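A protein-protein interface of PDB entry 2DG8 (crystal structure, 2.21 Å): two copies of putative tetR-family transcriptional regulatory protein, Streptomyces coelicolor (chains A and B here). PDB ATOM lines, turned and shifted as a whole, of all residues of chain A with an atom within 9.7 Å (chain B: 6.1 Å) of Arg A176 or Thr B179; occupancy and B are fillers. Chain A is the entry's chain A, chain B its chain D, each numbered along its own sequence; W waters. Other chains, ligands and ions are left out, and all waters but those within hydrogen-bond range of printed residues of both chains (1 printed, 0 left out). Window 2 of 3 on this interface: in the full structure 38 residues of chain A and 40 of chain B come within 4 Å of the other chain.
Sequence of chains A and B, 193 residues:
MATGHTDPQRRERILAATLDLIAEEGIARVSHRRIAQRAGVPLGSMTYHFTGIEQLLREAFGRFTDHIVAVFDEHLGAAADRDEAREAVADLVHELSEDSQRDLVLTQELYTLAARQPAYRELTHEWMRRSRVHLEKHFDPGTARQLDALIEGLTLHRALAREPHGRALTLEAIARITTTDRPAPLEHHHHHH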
ATOM      1  N   ARG A  86      12.382  -6.684   6.615  1.00  0.00           N
ATOM      2  CA  ARG A  86      11.109  -7.294   6.253  1.00  0.00           C
ATOM      3  C   ARG A  86      11.151  -7.746   4.800  1.00  0.00           C
ATOM      4  O   ARG A  86      10.686  -8.837   4.462  1.00  0.00           O
ATOM      5  CB  ARG A  86       9.954  -6.298   6.432  1.00  0.00           C
ATOM      6  CG  ARG A  86       9.742  -5.822   7.855  1.00  0.00           C
ATOM      7  CD  ARG A  86       8.505  -4.937   7.955  1.00  0.00           C
ATOM      8  NE  ARG A  86       8.190  -4.578   9.339  1.00  0.00           N
ATOM      9  CZ  ARG A  86       8.585  -3.457   9.943  1.00  0.00           C
ATOM     10  NH1 ARG A  86       8.242  -3.232  11.207  1.00  0.00           N
ATOM     11  NH2 ARG A  86       9.308  -2.556   9.285  1.00  0.00           N
ATOM     12  N   PHE A 139      14.780  -7.266  14.905  1.00  0.00           N
ATOM     13  CA  PHE A 139      13.536  -7.289  15.667  1.00  0.00           C
ATOM     14  C   PHE A 139      13.788  -7.752  17.089  1.00  0.00           C
ATOM     15  O   PHE A 139      14.783  -8.428  17.357  1.00  0.00           O
ATOM     16  CB  PHE A 139      12.530  -8.238  15.004  1.00  0.00           C
ATOM     17  CG  PHE A 139      12.279  -7.941  13.548  1.00  0.00           C
ATOM     18  CD1 PHE A 139      11.395  -6.936  13.170  1.00  0.00           C
ATOM     19  CD2 PHE A 139      12.958  -8.643  12.557  1.00  0.00           C
ATOM     20  CE1 PHE A 139      11.192  -6.633  11.824  1.00  0.00           C
ATOM     21  CE2 PHE A 139      12.765  -8.349  11.210  1.00  0.00           C
ATOM     22  CZ  PHE A 139      11.882  -7.341  10.844  1.00  0.00           C
ATOM     23  N   THR A 143       9.195 -10.933  18.782  1.00  0.00           N
ATOM     24  CA  THR A 143       8.754 -10.921  17.394  1.00  0.00           C
ATOM     25  C   THR A 143       9.656 -11.826  16.561  1.00  0.00           C
ATOM     26  O   THR A 143       9.195 -12.514  15.648  1.00  0.00           O
ATOM     27  CB  THR A 143       8.756  -9.496  16.806  1.00  0.00           C
ATOM     28  OG1 THR A 143      10.099  -9.082  16.549  1.00  0.00           O
ATOM     29  CG2 THR A 143       8.126  -8.531  17.781  1.00  0.00           C
ATOM     30  N   GLN A 146       8.287 -15.234  16.890  1.00  0.00           N
ATOM     31  CA  GLN A 146       7.035 -15.366  16.148  1.00  0.00           C
ATOM     32  C   GLN A 146       7.340 -15.369  14.642  1.00  0.00           C
ATOM     33  O   GLN A 146       6.757 -16.143  13.875  1.00  0.00           O
ATOM     34  CB  GLN A 146       6.088 -14.204  16.481  1.00  0.00           C
ATOM     35  CG  GLN A 146       5.789 -14.054  17.969  1.00  0.00           C
ATOM     36  CD  GLN A 146       4.971 -12.809  18.292  1.00  0.00           C
ATOM     37  OE1 GLN A 146       5.111 -12.230  19.372  1.00  0.00           O
ATOM     38  NE2 GLN A 146       4.106 -12.399  17.367  1.00  0.00           N
ATOM     39  N   LEU A 147       8.268 -14.510  14.234  1.00  0.00           N
ATOM     40  CA  LEU A 147       8.650 -14.400  12.832  1.00  0.00           C
ATOM     41  C   LEU A 147       9.304 -15.673  12.297  1.00  0.00           C
ATOM     42  O   LEU A 147       9.038 -16.081  11.162  1.00  0.00           O
ATOM     43  CB  LEU A 147       9.590 -13.203  12.638  1.00  0.00           C
ATOM     44  CG  LEU A 147      10.050 -12.909  11.213  1.00  0.00           C
ATOM     45  CD1 LEU A 147       8.847 -12.900  10.253  1.00  0.00           C
ATOM     46  CD2 LEU A 147      10.784 -11.566  11.198  1.00  0.00           C
ATOM     47  N   LEU A 150       6.728 -18.049  11.427  1.00  0.00           N
ATOM     48  CA  LEU A 150       6.000 -17.640  10.225  1.00  0.00           C
ATOM     49  C   LEU A 150       6.823 -18.023   9.001  1.00  0.00           C
ATOM     50  O   LEU A 150       6.301 -18.601   8.044  1.00  0.00           O
ATOM     51  CB  LEU A 150       5.740 -16.124  10.218  1.00  0.00           C
ATOM     52  CG  LEU A 150       5.018 -15.562   8.986  1.00  0.00           C
ATOM     53  CD1 LEU A 150       3.630 -16.198   8.877  1.00  0.00           C
ATOM     54  CD2 LEU A 150       4.896 -14.038   9.088  1.00  0.00           C
ATOM     55  N   LEU A 154       5.412 -20.240   6.005  1.00  0.00           N
ATOM     56  CA  LEU A 154       5.254 -19.671   4.665  1.00  0.00           C
ATOM     57  C   LEU A 154       6.102 -20.447   3.664  1.00  0.00           C
ATOM     58  O   LEU A 154       5.668 -20.730   2.554  1.00  0.00           O
ATOM     59  CB  LEU A 154       5.667 -18.185   4.644  1.00  0.00           C
ATOM     60  CG  LEU A 154       4.728 -17.159   5.302  1.00  0.00           C
ATOM     61  CD1 LEU A 154       5.395 -15.779   5.357  1.00  0.00           C
ATOM     62  CD2 LEU A 154       3.430 -17.075   4.520  1.00  0.00           C
ATOM     63  N   ALA A 168       3.562 -10.522  -2.457  1.00  0.00           N
ATOM     64  CA  ALA A 168       2.746  -9.524  -1.762  1.00  0.00           C
ATOM     65  C   ALA A 168       2.120 -10.140  -0.511  1.00  0.00           C
ATOM     66  O   ALA A 168       2.116  -9.538   0.561  1.00  0.00           O
ATOM     67  CB  ALA A 168       1.651  -8.986  -2.691  1.00  0.00           C
ATOM     68  N   LEU A 169       1.591 -11.349  -0.653  1.00  0.00           N
ATOM     69  CA  LEU A 169       0.986 -12.057   0.467  1.00  0.00           C
ATOM     70  C   LEU A 169       2.063 -12.378   1.505  1.00  0.00           C
ATOM     71  O   LEU A 169       1.827 -12.279   2.700  1.00  0.00           O
ATOM     72  CB  LEU A 169       0.323 -13.347  -0.036  1.00  0.00           C
ATOM     73  CG  LEU A 169      -0.534 -14.198   0.908  1.00  0.00           C
ATOM     74  CD1 LEU A 169       0.356 -14.956   1.877  1.00  0.00           C
ATOM     75  CD2 LEU A 169      -1.524 -13.313   1.635  1.00  0.00           C
ATOM     76  N   THR A 170       3.249 -12.765   1.045  1.00  0.00           N
ATOM     77  CA  THR A 170       4.343 -13.077   1.956  1.00  0.00           C
ATOM     78  C   THR A 170       4.761 -11.808   2.712  1.00  0.00           C
ATOM     79  O   THR A 170       4.924 -11.815   3.929  1.00  0.00           O
ATOM     80  CB  THR A 170       5.587 -13.640   1.202  1.00  0.00           C
ATOM     81  OG1 THR A 170       5.261 -14.898   0.584  1.00  0.00           O
ATOM     82  CG2 THR A 170       6.751 -13.862   2.187  1.00  0.00           C
ATOM     83  N   LEU A 171       4.912 -10.713   1.982  1.00  0.00           N
ATOM     84  CA  LEU A 171       5.328  -9.462   2.590  1.00  0.00           C
ATOM     85  C   LEU A 171       4.314  -8.943   3.604  1.00  0.00           C
ATOM     86  O   LEU A 171       4.693  -8.406   4.640  1.00  0.00           O
ATOM     87  CB  LEU A 171       5.573  -8.421   1.501  1.00  0.00           C
ATOM     88  CG  LEU A 171       6.415  -7.224   1.928  1.00  0.00           C
ATOM     89  CD1 LEU A 171       7.798  -7.691   2.409  1.00  0.00           C
ATOM     90  CD2 LEU A 171       6.541  -6.273   0.745  1.00  0.00           C
ATOM     91  N   GLU A 172       3.026  -9.116   3.321  1.00  0.00           N
ATOM     92  CA  GLU A 172       1.988  -8.657   4.242  1.00  0.00           C
ATOM     93  C   GLU A 172       2.013  -9.426   5.564  1.00  0.00           C
ATOM     94  O   GLU A 172       1.901  -8.834   6.631  1.00  0.00           O
ATOM     95  CB  GLU A 172       0.592  -8.788   3.616  1.00  0.00           C
ATOM     96  CG  GLU A 172      -0.484  -8.056   4.411  1.00  0.00           C
ATOM     97  CD  GLU A 172      -1.873  -8.218   3.827  1.00  0.00           C
ATOM     98  OE1 GLU A 172      -2.449  -9.322   3.936  1.00  0.00           O
ATOM     99  OE2 GLU A 172      -2.391  -7.239   3.248  1.00  0.00           O
ATOM    100  N   ALA A 173       2.142 -10.747   5.494  1.00  0.00           N
ATOM    101  CA  ALA A 173       2.170 -11.563   6.713  1.00  0.00           C
ATOM    102  C   ALA A 173       3.363 -11.128   7.552  1.00  0.00           C
ATOM    103  O   ALA A 173       3.276 -10.980   8.773  1.00  0.00           O
ATOM    104  CB  ALA A 173       2.286 -13.048   6.364  1.00  0.00           C
ATOM    105  N   ILE A 174       4.488 -10.919   6.884  1.00  0.00           N
ATOM    106  CA  ILE A 174       5.686 -10.489   7.573  1.00  0.00           C
ATOM    107  C   ILE A 174       5.444  -9.132   8.230  1.00  0.00           C
ATOM    108  O   ILE A 174       5.752  -8.950   9.410  1.00  0.00           O
ATOM    109  CB  ILE A 174       6.870 -10.426   6.587  1.00  0.00           C
ATOM    110  CG1 ILE A 174       7.233 -11.854   6.156  1.00  0.00           C
ATOM    111  CG2 ILE A 174       8.053  -9.725   7.228  1.00  0.00           C
ATOM    112  CD1 ILE A 174       8.069 -11.951   4.897  1.00  0.00           C
ATOM    113  N   ALA A 175       4.871  -8.191   7.483  1.00  0.00           N
ATOM    114  CA  ALA A 175       4.602  -6.868   8.039  1.00  0.00           C
ATOM    115  C   ALA A 175       3.702  -6.984   9.258  1.00  0.00           C
ATOM    116  O   ALA A 175       3.940  -6.340  10.274  1.00  0.00           O
ATOM    117  CB  ALA A 175       3.950  -5.957   6.986  1.00  0.00           C
ATOM    118  N   ARG A 176       2.670  -7.814   9.161  1.00  0.00           N
ATOM    119  CA  ARG A 176       1.750  -8.001  10.276  1.00  0.00           C
ATOM    120  C   ARG A 176       2.404  -8.623  11.525  1.00  0.00           C
ATOM    121  O   ARG A 176       2.265  -8.088  12.627  1.00  0.00           O
ATOM    122  CB  ARG A 176       0.531  -8.811   9.792  1.00  0.00           C
ATOM    123  CG  ARG A 176      -0.534  -7.895   9.168  1.00  0.00           C
ATOM    124  CD  ARG A 176      -1.362  -8.475   8.010  1.00  0.00           C
ATOM    125  NE  ARG A 176      -2.394  -9.419   8.416  1.00  0.00           N
ATOM    126  CZ  ARG A 176      -3.551  -9.590   7.776  1.00  0.00           C
ATOM    127  NH1 ARG A 176      -4.428 -10.482   8.217  1.00  0.00           N
ATOM    128  NH2 ARG A 176      -3.850  -8.861   6.711  1.00  0.00           N
ATOM    129  N   ILE A 177       3.148  -9.719  11.355  1.00  0.00           N
ATOM    130  CA  ILE A 177       3.809 -10.382  12.485  1.00  0.00           C
ATOM    131  C   ILE A 177       4.857  -9.470  13.156  1.00  0.00           C
ATOM    132  O   ILE A 177       5.075  -9.551  14.360  1.00  0.00           O
ATOM    133  CB  ILE A 177       4.499 -11.704  12.042  1.00  0.00           C
ATOM    134  CG1 ILE A 177       4.545 -12.700  13.201  1.00  0.00           C
ATOM    135  CG2 ILE A 177       5.930 -11.432  11.594  1.00  0.00           C
ATOM    136  CD1 ILE A 177       3.217 -13.307  13.553  1.00  0.00           C
ATOM    137  N   THR A 178       5.492  -8.598  12.380  1.00  0.00           N
ATOM    138  CA  THR A 178       6.499  -7.696  12.926  1.00  0.00           C
ATOM    139  C   THR A 178       5.924  -6.325  13.318  1.00  0.00           C
ATOM    140  O   THR A 178       6.644  -5.326  13.380  1.00  0.00           O
ATOM    141  CB  THR A 178       7.662  -7.493  11.928  1.00  0.00           C
ATOM    142  OG1 THR A 178       7.150  -6.979  10.698  1.00  0.00           O
ATOM    143  CG2 THR A 178       8.377  -8.819  11.654  1.00  0.00           C
ATOM    144  N   THR A 179       4.623  -6.276  13.578  1.00  0.00           N
ATOM    145  CA  THR A 179       3.988  -5.027  13.989  1.00  0.00           C
ATOM    146  C   THR A 179       3.904  -4.984  15.518  1.00  0.00           C
ATOM    147  O   THR A 179       3.501  -5.959  16.146  1.00  0.00           O
ATOM    148  CB  THR A 179       2.554  -4.897  13.421  1.00  0.00           C
ATOM    149  OG1 THR A 179       2.611  -4.625  12.017  1.00  0.00           O
ATOM    150  CG2 THR A 179       1.807  -3.776  14.123  1.00  0.00           C
ATOM    151  N   THR A 180       4.303  -3.860  16.105  1.00  0.00           N
ATOM    152  CA  THR A 180       4.250  -3.684  17.553  1.00  0.00           C
ATOM    153  C   THR A 180       3.679  -2.306  17.916  1.00  0.00           C
ATOM    154  O   THR A 180       4.312  -1.531  18.635  1.00  0.00           O
ATOM    155  CB  THR A 180       5.652  -3.834  18.191  1.00  0.00           C
ATOM    156  OG1 THR A 180       6.584  -2.992  17.503  1.00  0.00           O
ATOM    157  CG2 THR A 180       6.123  -5.277  18.120  1.00  0.00           C
ATOM    158  N   ASP A 181       2.485  -2.009  17.402  1.00  0.00           N
ATOM    159  CA  ASP A 181       1.794  -0.740  17.659  1.00  0.00           C
ATOM    160  C   ASP A 181       0.307  -1.002  17.877  1.00  0.00           C
ATOM    161  O   ASP A 181      -0.108  -2.164  17.677  1.00  0.00           O
ATOM    162  CB  ASP A 181       1.988   0.230  16.479  1.00  0.00           C
ATOM    163  CG  ASP A 181       1.008   1.415  16.507  1.00  0.00           C
ATOM    164  OD1 ASP A 181      -0.162   1.244  16.095  1.00  0.00           O
ATOM    165  OD2 ASP A 181       1.406   2.517  16.943  1.00  0.00           O
ATOM    166  N   ARG B  86      -9.673 -17.068  17.604  1.00  0.00           N
ATOM    167  CA  ARG B  86      -8.248 -16.936  17.884  1.00  0.00           C
ATOM    168  C   ARG B  86      -7.793 -17.895  18.981  1.00  0.00           C
ATOM    169  O   ARG B  86      -6.798 -18.601  18.819  1.00  0.00           O
ATOM    170  CB  ARG B  86      -7.925 -15.491  18.281  1.00  0.00           C
ATOM    171  CG  ARG B  86      -8.117 -14.507  17.141  1.00  0.00           C
ATOM    172  CD  ARG B  86      -7.747 -13.085  17.533  1.00  0.00           C
ATOM    173  NE  ARG B  86      -7.726 -12.211  16.363  1.00  0.00           N
ATOM    174  CZ  ARG B  86      -8.671 -11.327  16.058  1.00  0.00           C
ATOM    175  NH1 ARG B  86      -8.551 -10.586  14.965  1.00  0.00           N
ATOM    176  NH2 ARG B  86      -9.723 -11.169  16.852  1.00  0.00           N
ATOM    177  N   ASP B 140     -11.121 -13.303   6.764  1.00  0.00           N
ATOM    178  CA  ASP B 140     -11.156 -13.051   5.329  1.00  0.00           C
ATOM    179  C   ASP B 140     -10.169 -14.026   4.669  1.00  0.00           C
ATOM    180  O   ASP B 140      -9.319 -14.597   5.348  1.00  0.00           O
ATOM    181  CB  ASP B 140     -10.748 -11.605   5.028  1.00  0.00           C
ATOM    182  CG  ASP B 140      -9.309 -11.324   5.385  1.00  0.00           C
ATOM    183  OD1 ASP B 140      -9.046 -10.888   6.525  1.00  0.00           O
ATOM    184  OD2 ASP B 140      -8.438 -11.563   4.524  1.00  0.00           O
ATOM    185  N   GLY B 142      -7.429 -13.702   2.519  1.00  0.00           N
ATOM    186  CA  GLY B 142      -6.013 -13.431   2.668  1.00  0.00           C
ATOM    187  C   GLY B 142      -5.499 -13.776   4.054  1.00  0.00           C
ATOM    188  O   GLY B 142      -4.433 -14.384   4.204  1.00  0.00           O
ATOM    189  N   THR B 143      -6.262 -13.389   5.071  1.00  0.00           N
ATOM    190  CA  THR B 143      -5.886 -13.633   6.453  1.00  0.00           C
ATOM    191  C   THR B 143      -5.890 -15.124   6.765  1.00  0.00           C
ATOM    192  O   THR B 143      -4.981 -15.629   7.426  1.00  0.00           O
ATOM    193  CB  THR B 143      -6.833 -12.872   7.414  1.00  0.00           C
ATOM    194  OG1 THR B 143      -6.671 -11.463   7.208  1.00  0.00           O
ATOM    195  CG2 THR B 143      -6.516 -13.199   8.864  1.00  0.00           C
ATOM    196  N   GLN B 146      -2.650 -16.643   5.431  1.00  0.00           N
ATOM    197  CA  GLN B 146      -1.480 -16.280   6.232  1.00  0.00           C
ATOM    198  C   GLN B 146      -1.512 -17.035   7.557  1.00  0.00           C
ATOM    199  O   GLN B 146      -0.490 -17.501   8.060  1.00  0.00           O
ATOM    200  CB  GLN B 146      -1.465 -14.764   6.525  1.00  0.00           C
ATOM    201  CG  GLN B 146      -1.412 -13.869   5.292  1.00  0.00           C
ATOM    202  CD  GLN B 146      -1.558 -12.380   5.630  1.00  0.00           C
ATOM    203  OE1 GLN B 146      -0.842 -11.846   6.488  1.00  0.00           O
ATOM    204  NE2 GLN B 146      -2.475 -11.705   4.944  1.00  0.00           N
ATOM    205  N   ILE B 174      -0.788 -15.112  16.579  1.00  0.00           N
ATOM    206  CA  ILE B 174      -2.086 -15.245  15.938  1.00  0.00           C
ATOM    207  C   ILE B 174      -2.805 -13.896  15.917  1.00  0.00           C
ATOM    208  O   ILE B 174      -3.403 -13.508  14.913  1.00  0.00           O
ATOM    209  CB  ILE B 174      -2.936 -16.298  16.689  1.00  0.00           C
ATOM    210  CG1 ILE B 174      -2.259 -17.671  16.559  1.00  0.00           C
ATOM    211  CG2 ILE B 174      -4.352 -16.325  16.152  1.00  0.00           C
ATOM    212  CD1 ILE B 174      -2.926 -18.780  17.342  1.00  0.00           C
ATOM    213  N   ALA B 175      -2.715 -13.172  17.024  1.00  0.00           N
ATOM    214  CA  ALA B 175      -3.353 -11.868  17.134  1.00  0.00           C
ATOM    215  C   ALA B 175      -2.807 -10.894  16.095  1.00  0.00           C
ATOM    216  O   ALA B 175      -3.549 -10.092  15.528  1.00  0.00           O
ATOM    217  CB  ALA B 175      -3.153 -11.304  18.541  1.00  0.00           C
ATOM    218  N   ARG B 176      -1.509 -10.968  15.839  1.00  0.00           N
ATOM    219  CA  ARG B 176      -0.894 -10.074  14.870  1.00  0.00           C
ATOM    220  C   ARG B 176      -1.232 -10.425  13.423  1.00  0.00           C
ATOM    221  O   ARG B 176      -1.546  -9.546  12.620  1.00  0.00           O
ATOM    222  CB  ARG B 176       0.627 -10.070  15.052  1.00  0.00           C
ATOM    223  CG  ARG B 176       1.080  -9.673  16.459  1.00  0.00           C
ATOM    224  CD  ARG B 176       2.586  -9.496  16.513  1.00  0.00           C
ATOM    225  NE  ARG B 176       3.055  -9.280  17.875  1.00  0.00           N
ATOM    226  CZ  ARG B 176       4.315  -9.016  18.198  1.00  0.00           C
ATOM    227  NH1 ARG B 176       5.243  -8.933  17.249  1.00  0.00           N
ATOM    228  NH2 ARG B 176       4.647  -8.841  19.471  1.00  0.00           N
ATOM    229  N   ILE B 177      -1.169 -11.709  13.096  1.00  0.00           N
ATOM    230  CA  ILE B 177      -1.444 -12.166  11.743  1.00  0.00           C
ATOM    231  C   ILE B 177      -2.919 -11.977  11.372  1.00  0.00           C
ATOM    232  O   ILE B 177      -3.247 -11.795  10.203  1.00  0.00           O
ATOM    233  CB  ILE B 177      -1.021 -13.658  11.576  1.00  0.00           C
ATOM    234  CG1 ILE B 177      -0.503 -13.897  10.160  1.00  0.00           C
ATOM    235  CG2 ILE B 177      -2.188 -14.590  11.887  1.00  0.00           C
ATOM    236  CD1 ILE B 177       0.813 -13.197   9.877  1.00  0.00           C
ATOM    237  N   THR B 178      -3.804 -12.011  12.365  1.00  0.00           N
ATOM    238  CA  THR B 178      -5.227 -11.818  12.109  1.00  0.00           C
ATOM    239  C   THR B 178      -5.642 -10.370  12.380  1.00  0.00           C
ATOM    240  O   THR B 178      -6.824 -10.081  12.558  1.00  0.00           O
ATOM    241  CB  THR B 178      -6.109 -12.747  12.974  1.00  0.00           C
ATOM    242  OG1 THR B 178      -5.865 -12.494  14.363  1.00  0.00           O
ATOM    243  CG2 THR B 178      -5.819 -14.209  12.651  1.00  0.00           C
ATOM    244  N   THR B 179      -4.671  -9.463  12.410  1.00  0.00           N
ATOM    245  CA  THR B 179      -4.975  -8.056  12.642  1.00  0.00           C
ATOM    246  C   THR B 179      -5.479  -7.437  11.348  1.00  0.00           C
ATOM    247  O   THR B 179      -4.800  -7.488  10.321  1.00  0.00           O
ATOM    248  CB  THR B 179      -3.736  -7.287  13.146  1.00  0.00           C
ATOM    249  OG1 THR B 179      -3.455  -7.686  14.493  1.00  0.00           O
ATOM    250  CG2 THR B 179      -3.975  -5.782  13.101  1.00  0.00           C
ATOM    251  N   THR B 180      -6.681  -6.869  11.417  1.00  0.00           N
ATOM    252  CA  THR B 180      -7.339  -6.246  10.276  1.00  0.00           C
ATOM    253  C   THR B 180      -7.734  -7.287   9.238  1.00  0.00           C
ATOM    254  O   THR B 180      -8.937  -7.361   8.923  1.00  0.00           O
ATOM    255  CB  THR B 180      -6.445  -5.175   9.624  1.00  0.00           C
ATOM    256  OG1 THR B 180      -6.489  -3.983  10.416  1.00  0.00           O
ATOM    257  CG2 THR B 180      -6.921  -4.853   8.215  1.00  0.00           C
HETATM  258  O   HOH W   1      -6.705  -9.756   5.019  1.00  0.00           O
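NE2 of Gln A146 lies close to NE of Arg B176 (3.3 Å).
The side-chain carboxylate (OE1) of Glu A172 is in hydrogen-bond range of the side-chain amide nitrogen (NE2) of Gln B146 (2.6 Å).
The backbone NH (N) of Ala A173 sits close to the side-chain amide oxygen (OE1) of Gln B146, at 3.3 Å.
NH1 of Arg A176 lies within hydrogen-bond range of OG1 of Thr B143, 2.6 Å away.
The guanidinium group of Arg A176 lies within hydrogen-bond range of the side-chain amide oxygen of Gln B146 (3.5 Å).
NH1 of Arg A176 is in hydrogen-bond range of O of Ile B177.
The backbone carbonyl oxygen of Ile A177 sits at hydrogen-bond distance from the guanidinium group of Arg B176, at 3.0 Å.
Printed residues of chain B within 4 Å of Arg A176: Thr B143 (2.6 Å), Gln B146 (3.5 Å), Arg B176 (3.5 Å), Ile B177 (2.7 Å) and Thr B179 (3.5 Å).
Thr B179 touches just one residue of chain A: Arg A176.
Of chain A, only Arg A176 comes within 4 Å of Thr B143.
No residue of chain A comes within 4 Å of Thr B178.
Printed residues of chain B within 4 Å of Thr A180: Arg B176 (3.9 Å).
Printed residues of chain B within 4 Å of Thr A179: Arg B176 (3.6 Å).
Of the printed residues of chain A, Ile B177 touches Ala A173 (3.5 Å) and Arg A176 (2.7 Å).
The nearest residue of chain B that does not touch Arg A176 is Thr B178 (4.2 Å).
Printed residues of chain B that touch a printed residue of chain A: Thr B143, Gln B146, Arg B176, Ile B177 and Thr B179.
Hydrophobic or aromatic side chains of chain B within 4 Å of the printed part of chain A: Ile B177.
Of the 21 printed residues of chain A, 9 touch a printed residue of chain B.
Hydrophobic or aromatic side chains of chain A that line the printed part of chain B: Leu A169 and Ala A173.
Gln A146 touches Arg B176, and with the chains exchanged Arg A176 touches Gln B146.
Arg B176 touches its own counterpart, Arg A176.
Arg A176 touches Ile B177, and with the chains exchanged Ile A177 touches Arg B176.
Arg A176 touches Thr B179, and with the chains exchanged Thr A179 touches Arg B176.
10 positions are printed for both chains.
Of the 14 pairs that touch across the chains among the printed residues, 9 have their exchanged pair printed and touching as well.
Water W1 lies within hydrogen-bond range of OD2 of Asp B140 (2.6 Å), OG1 of Thr B143 (2.8 Å) and NH2 of Arg A176 (3.4 Å).
CG2 of Thr A143 touches NH1 of Arg B176, at 3.0 Å.
Gln B146 touches Leu A169 (CG to CD2, 3.7 Å).
Ile B177 touches Ala A173 (CD1 to O, 3.5 Å).
Arg A176 touches Arg B176.
Arg A176 touches Thr B179 (CZ to O, 3.5 Å).
Thr A179 touches Arg B176.
Thr A180 touches Arg B176.
The side-chain carboxylate of Glu A172 is in salt-bridge range of the guanidinium group of Arg A176 (3.1 Å).
The side-chain hydroxyl of Thr A179 sits at hydrogen-bond distance from the backbone carbonyl oxygen of Ala A175, 2.8 Å away.
The side-chain carboxylate (OD1) of Asp B140 is in hydrogen-bond range of the side-chain hydroxyl (OG1) of Thr B143 (2.5 Å).
The backbone carbonyl oxygen of Gly B142 sits close to the side-chain amide nitrogen of Gln B146.
O of Ala B175 lies within hydrogen-bond range of OG1 of Thr B179, 2.6 Å away.
The side-chain hydroxyl (OG1) of Thr B179 sits close to the backbone carbonyl oxygen (O) of Arg B176.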
